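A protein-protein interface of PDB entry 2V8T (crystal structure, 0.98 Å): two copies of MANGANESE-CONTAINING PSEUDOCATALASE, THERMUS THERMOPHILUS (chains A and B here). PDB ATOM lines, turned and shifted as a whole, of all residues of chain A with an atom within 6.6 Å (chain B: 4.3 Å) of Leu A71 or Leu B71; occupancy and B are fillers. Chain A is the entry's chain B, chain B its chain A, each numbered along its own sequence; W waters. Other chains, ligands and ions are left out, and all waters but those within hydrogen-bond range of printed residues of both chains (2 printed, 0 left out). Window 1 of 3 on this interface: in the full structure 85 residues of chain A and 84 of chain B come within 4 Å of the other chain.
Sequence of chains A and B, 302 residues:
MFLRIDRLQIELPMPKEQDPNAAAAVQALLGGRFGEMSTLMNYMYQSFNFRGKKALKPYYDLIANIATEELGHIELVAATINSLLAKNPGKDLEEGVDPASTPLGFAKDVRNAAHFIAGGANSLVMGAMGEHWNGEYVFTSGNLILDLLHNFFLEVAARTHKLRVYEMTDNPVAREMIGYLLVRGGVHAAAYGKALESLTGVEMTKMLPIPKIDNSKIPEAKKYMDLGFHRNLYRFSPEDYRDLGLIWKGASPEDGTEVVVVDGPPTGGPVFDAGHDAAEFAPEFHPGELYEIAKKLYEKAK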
ATOM      1  N   MET A   1      27.957 -14.032  36.382  1.00  0.00           N
ATOM      2  CA  MET A   1      29.056 -14.762  35.680  1.00  0.00           C
ATOM      3  C   MET A   1      28.409 -15.736  34.723  1.00  0.00           C
ATOM      4  O   MET A   1      27.189 -15.982  34.827  1.00  0.00           O
ATOM      5  CB  MET A   1      29.987 -15.496  36.649  1.00  0.00           C
ATOM      6  CG  MET A   1      30.971 -14.597  37.369  1.00  0.00           C
ATOM      7  SD  MET A   1      32.073 -15.516  38.462  1.00  0.00           S
ATOM      8  CE  MET A   1      30.997 -15.771  39.826  1.00  0.00           C
ATOM      9  N   PHE A   2      29.201 -16.329  33.841  1.00  0.00           N
ATOM     10  CA  PHE A   2      28.726 -17.228  32.831  1.00  0.00           C
ATOM     11  C   PHE A   2      29.619 -18.447  32.698  1.00  0.00           C
ATOM     12  O   PHE A   2      30.830 -18.389  33.003  1.00  0.00           O
ATOM     13  CB  PHE A   2      28.621 -16.492  31.472  1.00  0.00           C
ATOM     14  CG  PHE A   2      27.593 -15.392  31.513  1.00  0.00           C
ATOM     15  CD1 PHE A   2      27.898 -14.136  32.035  1.00  0.00           C
ATOM     16  CD2 PHE A   2      26.294 -15.630  31.054  1.00  0.00           C
ATOM     17  CE1 PHE A   2      26.901 -13.148  32.117  1.00  0.00           C
ATOM     18  CE2 PHE A   2      25.321 -14.648  31.108  1.00  0.00           C
ATOM     19  CZ  PHE A   2      25.615 -13.422  31.664  1.00  0.00           C
ATOM     20  N   LEU A   3      29.030 -19.524  32.185  1.00  0.00           N
ATOM     21  CA  LEU A   3      29.746 -20.737  31.815  1.00  0.00           C
ATOM     22  C   LEU A   3      29.448 -21.037  30.340  1.00  0.00           C
ATOM     23  O   LEU A   3      28.426 -20.564  29.797  1.00  0.00           O
ATOM     24  CB  LEU A   3      29.299 -21.941  32.635  1.00  0.00           C
ATOM     25  CG  LEU A   3      29.375 -21.778  34.155  1.00  0.00           C
ATOM     26  CD1 LEU A   3      28.740 -23.013  34.821  1.00  0.00           C
ATOM     27  CD2 LEU A   3      30.838 -21.572  34.614  1.00  0.00           C
ATOM     28  N   GLU A  36      20.447 -11.190  16.166  1.00  0.00           N
ATOM     29  CA  GLU A  36      20.621 -11.817  17.455  1.00  0.00           C
ATOM     30  C   GLU A  36      21.548 -11.026  18.363  1.00  0.00           C
ATOM     31  O   GLU A  36      21.418 -11.073  19.581  1.00  0.00           O
ATOM     32  CB  GLU A  36      21.144 -13.274  17.236  1.00  0.00           C
ATOM     33  CG  GLU A  36      20.067 -14.180  16.613  1.00  0.00           C
ATOM     34  CD  GLU A  36      18.976 -14.551  17.578  1.00  0.00           C
ATOM     35  OE1 GLU A  36      19.074 -14.268  18.748  1.00  0.00           O
ATOM     36  OE2 GLU A  36      17.957 -15.167  17.189  1.00  0.00           O
ATOM     37  N   LEU A  40      20.217 -10.267  22.108  1.00  0.00           N
ATOM     38  CA  LEU A  40      21.191 -10.558  23.156  1.00  0.00           C
ATOM     39  C   LEU A  40      21.493  -9.326  24.004  1.00  0.00           C
ATOM     40  O   LEU A  40      21.416  -9.349  25.226  1.00  0.00           O
ATOM     41  CB  LEU A  40      22.490 -11.074  22.537  1.00  0.00           C
ATOM     42  CG  LEU A  40      23.691 -11.142  23.492  1.00  0.00           C
ATOM     43  CD1 LEU A  40      23.424 -12.087  24.666  1.00  0.00           C
ATOM     44  CD2 LEU A  40      24.934 -11.571  22.693  1.00  0.00           C
ATOM     45  N   MET A  41      21.963  -8.243  23.348  1.00  0.00           N
ATOM     46  CA  MET A  41      22.495  -7.136  24.132  1.00  0.00           C
ATOM     47  C   MET A  41      21.412  -6.337  24.817  1.00  0.00           C
ATOM     48  O   MET A  41      21.606  -5.797  25.910  1.00  0.00           O
ATOM     49  CB  MET A  41      23.431  -6.282  23.278  1.00  0.00           C
ATOM     50  CG  MET A  41      24.704  -7.017  22.891  1.00  0.00           C
ATOM     51  SD  MET A  41      25.764  -7.313  24.331  1.00  0.00           S
ATOM     52  CE  MET A  41      26.986  -8.368  23.690  1.00  0.00           C
ATOM     53  N   MET A  44      20.642  -8.548  27.822  1.00  0.00           N
ATOM     54  CA  MET A  44      21.786  -8.589  28.717  1.00  0.00           C
ATOM     55  C   MET A  44      21.873  -7.294  29.529  1.00  0.00           C
ATOM     56  O   MET A  44      21.982  -7.319  30.751  1.00  0.00           O
ATOM     57  CB  MET A  44      23.073  -8.841  27.941  1.00  0.00           C
ATOM     58  CG  MET A  44      24.224  -9.209  28.752  1.00  0.00           C
ATOM     59  SD  MET A  44      24.067 -10.709  29.734  1.00  0.00           S
ATOM     60  CE  MET A  44      24.152 -11.825  28.573  1.00  0.00           C
ATOM     61  N   PHE A  48      21.435  -6.506  33.565  1.00  0.00           N
ATOM     62  CA  PHE A  48      22.402  -5.840  34.429  1.00  0.00           C
ATOM     63  C   PHE A  48      21.735  -4.698  35.179  1.00  0.00           C
ATOM     64  O   PHE A  48      21.934  -4.479  36.386  1.00  0.00           O
ATOM     65  CB  PHE A  48      23.579  -5.302  33.623  1.00  0.00           C
ATOM     66  CG  PHE A  48      24.395  -6.328  32.872  1.00  0.00           C
ATOM     67  CD1 PHE A  48      24.396  -7.691  33.173  1.00  0.00           C
ATOM     68  CD2 PHE A  48      25.204  -5.890  31.801  1.00  0.00           C
ATOM     69  CE1 PHE A  48      25.182  -8.585  32.473  1.00  0.00           C
ATOM     70  CE2 PHE A  48      26.026  -6.792  31.137  1.00  0.00           C
ATOM     71  CZ  PHE A  48      26.007  -8.133  31.468  1.00  0.00           C
ATOM     72  N   ILE A  66      16.520 -15.285  29.311  1.00  0.00           N
ATOM     73  CA  ILE A  66      16.419 -15.174  27.854  1.00  0.00           C
ATOM     74  C   ILE A  66      17.708 -14.541  27.298  1.00  0.00           C
ATOM     75  O   ILE A  66      18.189 -14.964  26.245  1.00  0.00           O
ATOM     76  CB  ILE A  66      15.117 -14.479  27.402  1.00  0.00           C
ATOM     77  CG1 ILE A  66      13.910 -15.338  27.783  1.00  0.00           C
ATOM     78  CG2 ILE A  66      15.139 -14.256  25.886  1.00  0.00           C
ATOM     79  CD1 ILE A  66      12.565 -14.721  27.474  1.00  0.00           C
ATOM     80  N   ALA A  67      18.283 -13.564  28.000  1.00  0.00           N
ATOM     81  CA  ALA A  67      19.586 -13.020  27.566  1.00  0.00           C
ATOM     82  C   ALA A  67      20.596 -14.143  27.370  1.00  0.00           C
ATOM     83  O   ALA A  67      21.376 -14.143  26.411  1.00  0.00           O
ATOM     84  CB  ALA A  67      20.109 -12.050  28.625  1.00  0.00           C
ATOM     85  N   THR A  68      20.625 -15.082  28.305  1.00  0.00           N
ATOM     86  CA  THR A  68      21.585 -16.181  28.245  1.00  0.00           C
ATOM     87  C   THR A  68      21.312 -17.085  27.046  1.00  0.00           C
ATOM     88  O   THR A  68      22.238 -17.526  26.368  1.00  0.00           O
ATOM     89  CB  THR A  68      21.572 -16.958  29.566  1.00  0.00           C
ATOM     90  OG1 THR A  68      21.752 -16.044  30.640  1.00  0.00           O
ATOM     91  CG2 THR A  68      22.678 -17.997  29.608  1.00  0.00           C
ATOM     92  N   GLU A  69      20.020 -17.371  26.754  1.00  0.00           N
ATOM     93  CA  GLU A  69      19.714 -18.134  25.564  1.00  0.00           C
ATOM     94  C   GLU A  69      20.248 -17.421  24.288  1.00  0.00           C
ATOM     95  O   GLU A  69      20.776 -18.062  23.378  1.00  0.00           O
ATOM     96  CB  GLU A  69      18.201 -18.412  25.403  1.00  0.00           C
ATOM     97  CG  GLU A  69      17.975 -19.266  24.165  1.00  0.00           C
ATOM     98  CD  GLU A  69      16.577 -19.825  23.913  1.00  0.00           C
ATOM     99  OE1 GLU A  69      15.645 -19.552  24.715  1.00  0.00           O
ATOM    100  OE2 GLU A  69      16.443 -20.512  22.856  1.00  0.00           O
ATOM    101  N   GLU A  70      20.069 -16.089  24.244  1.00  0.00           N
ATOM    102  CA  GLU A  70      20.482 -15.370  23.026  1.00  0.00           C
ATOM    103  C   GLU A  70      21.988 -15.467  22.794  1.00  0.00           C
ATOM    104  O   GLU A  70      22.431 -15.335  21.641  1.00  0.00           O
ATOM    105  CB  GLU A  70      20.041 -13.900  23.058  1.00  0.00           C
ATOM    106  CG  GLU A  70      18.566 -13.623  23.249  1.00  0.00           C
ATOM    107  CD  GLU A  70      17.599 -14.082  22.174  1.00  0.00           C
ATOM    108  OE1 GLU A  70      17.968 -14.892  21.346  1.00  0.00           O
ATOM    109  OE2 GLU A  70      16.400 -13.691  22.246  1.00  0.00           O
ATOM    110  N   LEU A  71      22.802 -15.696  23.818  1.00  0.00           N
ATOM    111  CA  LEU A  71      24.252 -15.953  23.596  1.00  0.00           C
ATOM    112  C   LEU A  71      24.431 -17.127  22.659  1.00  0.00           C
ATOM    113  O   LEU A  71      25.293 -17.109  21.767  1.00  0.00           O
ATOM    114  CB  LEU A  71      24.966 -16.250  24.921  1.00  0.00           C
ATOM    115  CG  LEU A  71      25.194 -15.066  25.858  1.00  0.00           C
ATOM    116  CD1 LEU A  71      25.610 -15.551  27.231  1.00  0.00           C
ATOM    117  CD2 LEU A  71      26.263 -14.138  25.295  1.00  0.00           C
ATOM    118  N   GLY A  72      23.686 -18.197  22.890  1.00  0.00           N
ATOM    119  CA  GLY A  72      23.762 -19.343  22.002  1.00  0.00           C
ATOM    120  C   GLY A  72      23.194 -19.087  20.638  1.00  0.00           C
ATOM    121  O   GLY A  72      23.529 -19.792  19.670  1.00  0.00           O
ATOM    122  N   HIS A  73      22.329 -18.089  20.489  1.00  0.00           N
ATOM    123  CA  HIS A  73      21.819 -17.735  19.171  1.00  0.00           C
ATOM    124  C   HIS A  73      22.822 -16.943  18.353  1.00  0.00           C
ATOM    125  O   HIS A  73      22.904 -17.202  17.152  1.00  0.00           O
ATOM    126  CB  HIS A  73      20.499 -16.997  19.267  1.00  0.00           C
ATOM    127  CG  HIS A  73      19.386 -17.825  19.837  1.00  0.00           C
ATOM    128  ND1 HIS A  73      18.100 -17.340  19.870  1.00  0.00           N
ATOM    129  CD2 HIS A  73      19.407 -19.053  20.422  1.00  0.00           C
ATOM    130  CE1 HIS A  73      17.371 -18.283  20.455  1.00  0.00           C
ATOM    131  NE2 HIS A  73      18.118 -19.322  20.797  1.00  0.00           N
ATOM    132  N   ILE A  74      23.569 -16.021  18.950  1.00  0.00           N
ATOM    133  CA  ILE A  74      24.645 -15.411  18.140  1.00  0.00           C
ATOM    134  C   ILE A  74      25.618 -16.495  17.682  1.00  0.00           C
ATOM    135  O   ILE A  74      26.100 -16.482  16.555  1.00  0.00           O
ATOM    136  CB  ILE A  74      25.362 -14.209  18.803  1.00  0.00           C
ATOM    137  CG1 ILE A  74      26.129 -14.520  20.072  1.00  0.00           C
ATOM    138  CG2 ILE A  74      24.399 -13.042  19.006  1.00  0.00           C
ATOM    139  CD1 ILE A  74      27.164 -13.445  20.434  1.00  0.00           C
ATOM    140  N   GLU A  75      25.879 -17.462  18.569  1.00  0.00           N
ATOM    141  CA  GLU A  75      26.777 -18.578  18.212  1.00  0.00           C
ATOM    142  C   GLU A  75      26.215 -19.368  17.048  1.00  0.00           C
ATOM    143  O   GLU A  75      26.929 -19.750  16.104  1.00  0.00           O
ATOM    144  CB  GLU A  75      26.929 -19.448  19.476  1.00  0.00           C
ATOM    145  CG  GLU A  75      27.880 -20.599  19.313  1.00  0.00           C
ATOM    146  CD  GLU A  75      27.982 -21.538  20.501  1.00  0.00           C
ATOM    147  OE1 GLU A  75      27.062 -21.489  21.384  1.00  0.00           O
ATOM    148  OE2 GLU A  75      28.956 -22.317  20.527  1.00  0.00           O
ATOM    149  N   LEU A  76      24.903 -19.691  17.098  1.00  0.00           N
ATOM    150  CA  LEU A  76      24.273 -20.515  16.061  1.00  0.00           C
ATOM    151  C   LEU A  76      24.245 -19.787  14.718  1.00  0.00           C
ATOM    152  O   LEU A  76      24.469 -20.388  13.663  1.00  0.00           O
ATOM    153  CB  LEU A  76      22.862 -20.892  16.515  1.00  0.00           C
ATOM    154  CG  LEU A  76      22.137 -21.906  15.630  1.00  0.00           C
ATOM    155  CD1 LEU A  76      22.828 -23.285  15.705  1.00  0.00           C
ATOM    156  CD2 LEU A  76      20.687 -22.039  16.032  1.00  0.00           C
ATOM    157  N   PHE B   2      25.571 -21.323  26.458  1.00  0.00           N
ATOM    158  CA  PHE B   2      26.030 -20.686  27.666  1.00  0.00           C
ATOM    159  C   PHE B   2      25.052 -20.873  28.808  1.00  0.00           C
ATOM    160  O   PHE B   2      23.840 -21.067  28.589  1.00  0.00           O
ATOM    161  CB  PHE B   2      26.251 -19.171  27.419  1.00  0.00           C
ATOM    162  CG  PHE B   2      27.350 -18.921  26.420  1.00  0.00           C
ATOM    163  CD1 PHE B   2      27.128 -19.008  25.052  1.00  0.00           C
ATOM    164  CD2 PHE B   2      28.665 -18.674  26.874  1.00  0.00           C
ATOM    165  CE1 PHE B   2      28.187 -18.840  24.146  1.00  0.00           C
ATOM    166  CE2 PHE B   2      29.698 -18.477  25.994  1.00  0.00           C
ATOM    167  CZ  PHE B   2      29.451 -18.583  24.627  1.00  0.00           C
ATOM    168  N   LEU B  40      35.468  -8.995  25.075  1.00  0.00           N
ATOM    169  CA  LEU B  40      34.425 -10.007  24.957  1.00  0.00           C
ATOM    170  C   LEU B  40      34.175 -10.362  23.517  1.00  0.00           C
ATOM    171  O   LEU B  40      34.189 -11.546  23.124  1.00  0.00           O
ATOM    172  CB  LEU B  40      33.140  -9.497  25.591  1.00  0.00           C
ATOM    173  CG  LEU B  40      31.907 -10.333  25.302  1.00  0.00           C
ATOM    174  CD1 LEU B  40      32.038 -11.755  25.810  1.00  0.00           C
ATOM    175  CD2 LEU B  40      30.670  -9.633  25.889  1.00  0.00           C
ATOM    176  N   ALA B  67      36.878 -15.772  26.348  1.00  0.00           N
ATOM    177  CA  ALA B  67      35.666 -15.090  25.922  1.00  0.00           C
ATOM    178  C   ALA B  67      34.586 -15.190  27.012  1.00  0.00           C
ATOM    179  O   ALA B  67      33.856 -14.240  27.296  1.00  0.00           O
ATOM    180  CB  ALA B  67      35.131 -15.697  24.637  1.00  0.00           C
ATOM    181  N   THR B  68      34.428 -16.404  27.568  1.00  0.00           N
ATOM    182  CA  THR B  68      33.407 -16.624  28.590  1.00  0.00           C
ATOM    183  C   THR B  68      33.671 -15.778  29.828  1.00  0.00           C
ATOM    184  O   THR B  68      32.764 -15.216  30.422  1.00  0.00           O
ATOM    185  CB  THR B  68      33.312 -18.112  28.929  1.00  0.00           C
ATOM    186  OG1 THR B  68      33.175 -18.836  27.717  1.00  0.00           O
ATOM    187  CG2 THR B  68      32.123 -18.395  29.823  1.00  0.00           C
ATOM    188  N   GLU B  69      34.952 -15.709  30.256  1.00  0.00           N
ATOM    189  CA  GLU B  69      35.272 -14.859  31.389  1.00  0.00           C
ATOM    190  C   GLU B  69      34.866 -13.390  31.099  1.00  0.00           C
ATOM    191  O   GLU B  69      34.357 -12.691  31.981  1.00  0.00           O
ATOM    192  CB  GLU B  69      36.769 -14.919  31.756  1.00  0.00           C
ATOM    193  CG  GLU B  69      37.013 -14.051  32.976  1.00  0.00           C
ATOM    194  CD  GLU B  69      38.387 -14.096  33.615  1.00  0.00           C
ATOM    195  OE1 GLU B  69      39.287 -14.844  33.149  1.00  0.00           O
ATOM    196  OE2 GLU B  69      38.559 -13.316  34.598  1.00  0.00           O
ATOM    197  N   GLU B  70      35.125 -12.914  29.867  1.00  0.00           N
ATOM    198  CA  GLU B  70      34.819 -11.512  29.573  1.00  0.00           C
ATOM    199  C   GLU B  70      33.335 -11.218  29.660  1.00  0.00           C
ATOM    200  O   GLU B  70      32.960 -10.045  29.913  1.00  0.00           O
ATOM    201  CB  GLU B  70      35.362 -11.103  28.196  1.00  0.00           C
ATOM    202  CG  GLU B  70      36.847 -11.308  27.932  1.00  0.00           C
ATOM    203  CD  GLU B  70      37.837 -10.503  28.775  1.00  0.00           C
ATOM    204  OE1 GLU B  70      37.460  -9.992  29.794  1.00  0.00           O
ATOM    205  OE2 GLU B  70      39.033 -10.506  28.413  1.00  0.00           O
ATOM    206  N   LEU B  71      32.447 -12.199  29.518  1.00  0.00           N
ATOM    207  CA  LEU B  71      31.016 -11.955  29.766  1.00  0.00           C
ATOM    208  C   LEU B  71      30.800 -11.427  31.173  1.00  0.00           C
ATOM    209  O   LEU B  71      29.989 -10.526  31.415  1.00  0.00           O
ATOM    210  CB  LEU B  71      30.191 -13.248  29.568  1.00  0.00           C
ATOM    211  CG  LEU B  71      30.012 -13.720  28.139  1.00  0.00           C
ATOM    212  CD1 LEU B  71      29.498 -15.168  28.128  1.00  0.00           C
ATOM    213  CD2 LEU B  71      29.046 -12.821  27.393  1.00  0.00           C
ATOM    214  N   GLY B  72      31.453 -12.054  32.156  1.00  0.00           N
ATOM    215  CA  GLY B  72      31.340 -11.592  33.508  1.00  0.00           C
ATOM    216  C   GLY B  72      31.991 -10.263  33.741  1.00  0.00           C
ATOM    217  O   GLY B  72      31.679  -9.556  34.718  1.00  0.00           O
ATOM    218  N   HIS B  73      32.932  -9.868  32.873  1.00  0.00           N
ATOM    219  CA  HIS B  73      33.536  -8.548  33.004  1.00  0.00           C
ATOM    220  C   HIS B  73      32.627  -7.442  32.489  1.00  0.00           C
ATOM    221  O   HIS B  73      32.580  -6.378  33.117  1.00  0.00           O
ATOM    222  CB  HIS B  73      34.899  -8.493  32.350  1.00  0.00           C
ATOM    223  CG  HIS B  73      35.895  -9.375  32.969  1.00  0.00           C
ATOM    224  ND1 HIS B  73      37.218  -9.362  32.567  1.00  0.00           N
ATOM    225  CD2 HIS B  73      35.755 -10.303  33.973  1.00  0.00           C
ATOM    226  CE1 HIS B  73      37.826 -10.287  33.308  1.00  0.00           C
ATOM    227  NE2 HIS B  73      36.974 -10.867  34.166  1.00  0.00           N
ATOM    228  N   ILE B  74      31.908  -7.630  31.377  1.00  0.00           N
ATOM    229  CA  ILE B  74      30.924  -6.604  31.025  1.00  0.00           C
ATOM    230  C   ILE B  74      29.925  -6.465  32.154  1.00  0.00           C
ATOM    231  O   ILE B  74      29.476  -5.362  32.487  1.00  0.00           O
ATOM    232  CB  ILE B  74      30.252  -6.780  29.634  1.00  0.00           C
ATOM    233  CG1 ILE B  74      29.419  -8.030  29.475  1.00  0.00           C
ATOM    234  CG2 ILE B  74      31.288  -6.658  28.526  1.00  0.00           C
ATOM    235  CD1 ILE B  74      28.432  -7.954  28.290  1.00  0.00           C
ATOM    236  N   GLU B  75      29.541  -7.594  32.770  1.00  0.00           N
ATOM    237  CA  GLU B  75      28.600  -7.574  33.896  1.00  0.00           C
ATOM    238  C   GLU B  75      29.158  -6.757  35.059  1.00  0.00           C
ATOM    239  O   GLU B  75      28.468  -5.944  35.668  1.00  0.00           O
ATOM    240  CB  GLU B  75      28.321  -9.035  34.291  1.00  0.00           C
ATOM    241  CG  GLU B  75      27.313  -9.153  35.395  1.00  0.00           C
ATOM    242  CD  GLU B  75      27.114 -10.589  35.895  1.00  0.00           C
ATOM    243  OE1 GLU B  75      28.011 -11.464  35.604  1.00  0.00           O
ATOM    244  OE2 GLU B  75      26.089 -10.805  36.579  1.00  0.00           O
HETATM  245  O   HOH W   1      23.044 -20.177  25.719  1.00  0.00           O
HETATM  246  O   HOH W   2      31.756 -15.247  33.177  1.00  0.00           O
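N of Met A1 sits at hydrogen-bond distance from OE1 of Glu B75 (2.7 Å).
Phe A2 touches Thr B68 (O to CG2, 3.4 Å).
Leu B71 touches Phe A2.
Leu A3 touches Phe B2 (O to CA, 3.2 Å).
C of Leu A3 touches CG2 of Thr B68, 3.8 Å away.
CE2 of Phe A48 touches CD1 of Ile B74, at 3.9 Å.
Glu B75 touches Phe A48 (CA to CZ, 3.6 Å).
Phe B2 touches Thr A68.
Leu A71 touches Phe B2 (CB to CD1, 3.5 Å).
Leu B71 touches Leu A71 (CD2 to CD2, 3.7 Å).
Glu A75 touches Phe B2.
Of the printed residues of chain B, Phe A2 touches Thr B68 (3.4 Å) and Leu B71 (3.5 Å).
Printed residues of chain B within 4 Å of Thr A68: Phe B2 (3.4 Å).
Of the printed residues of chain A, Thr B68 touches Phe A2 and Leu A3.
Glu B70 touches none of the printed residues of chain A.
The nearest printed residue of chain B that does not touch Leu A71 is Leu B40 (6.3 Å).
The nearest residue of chain A that does not touch Leu B71 is Phe A48 (4.6 Å).
The nearest printed residue of chain B that does not touch Met A1 is Gly B72 (4.5 Å).
Of the 11 printed residues of chain B, 5 touch a printed residue of chain A.
Among the printed residues, no Asp or Glu carboxylate lies within 4 Å of a Lys or Arg side-chain nitrogen of the other chain.
Phe A2 touches Thr B68, and with the chains exchanged Thr A68 touches Phe B2.
Phe A2 touches Leu B71, and with the chains exchanged Leu A71 touches Phe B2.
Leu A71 touches its own counterpart, Leu B71.
Glu A75 touches Phe B2, but with the chains exchanged Phe A2 does not touch Glu B75 (4.03 Å).
Positions printed for both chains: 2, 40, 67, 68, 69, 70, 71, 72, 73, 74 and 75.
Of the 11 pairs that touch across the chains among the printed residues, 5 have their exchanged pair printed and touching as well.
Water W1 bridges O of Thr A68 (2.8 Å) and N of Phe B2 (2.9 Å).
Water W2 lies within hydrogen-bond range of the backbone NH of Phe A2 (2.9 Å), the backbone carbonyl oxygen of Thr B68 (2.9 Å) and the backbone NH of Gly B72 (3.4 Å).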
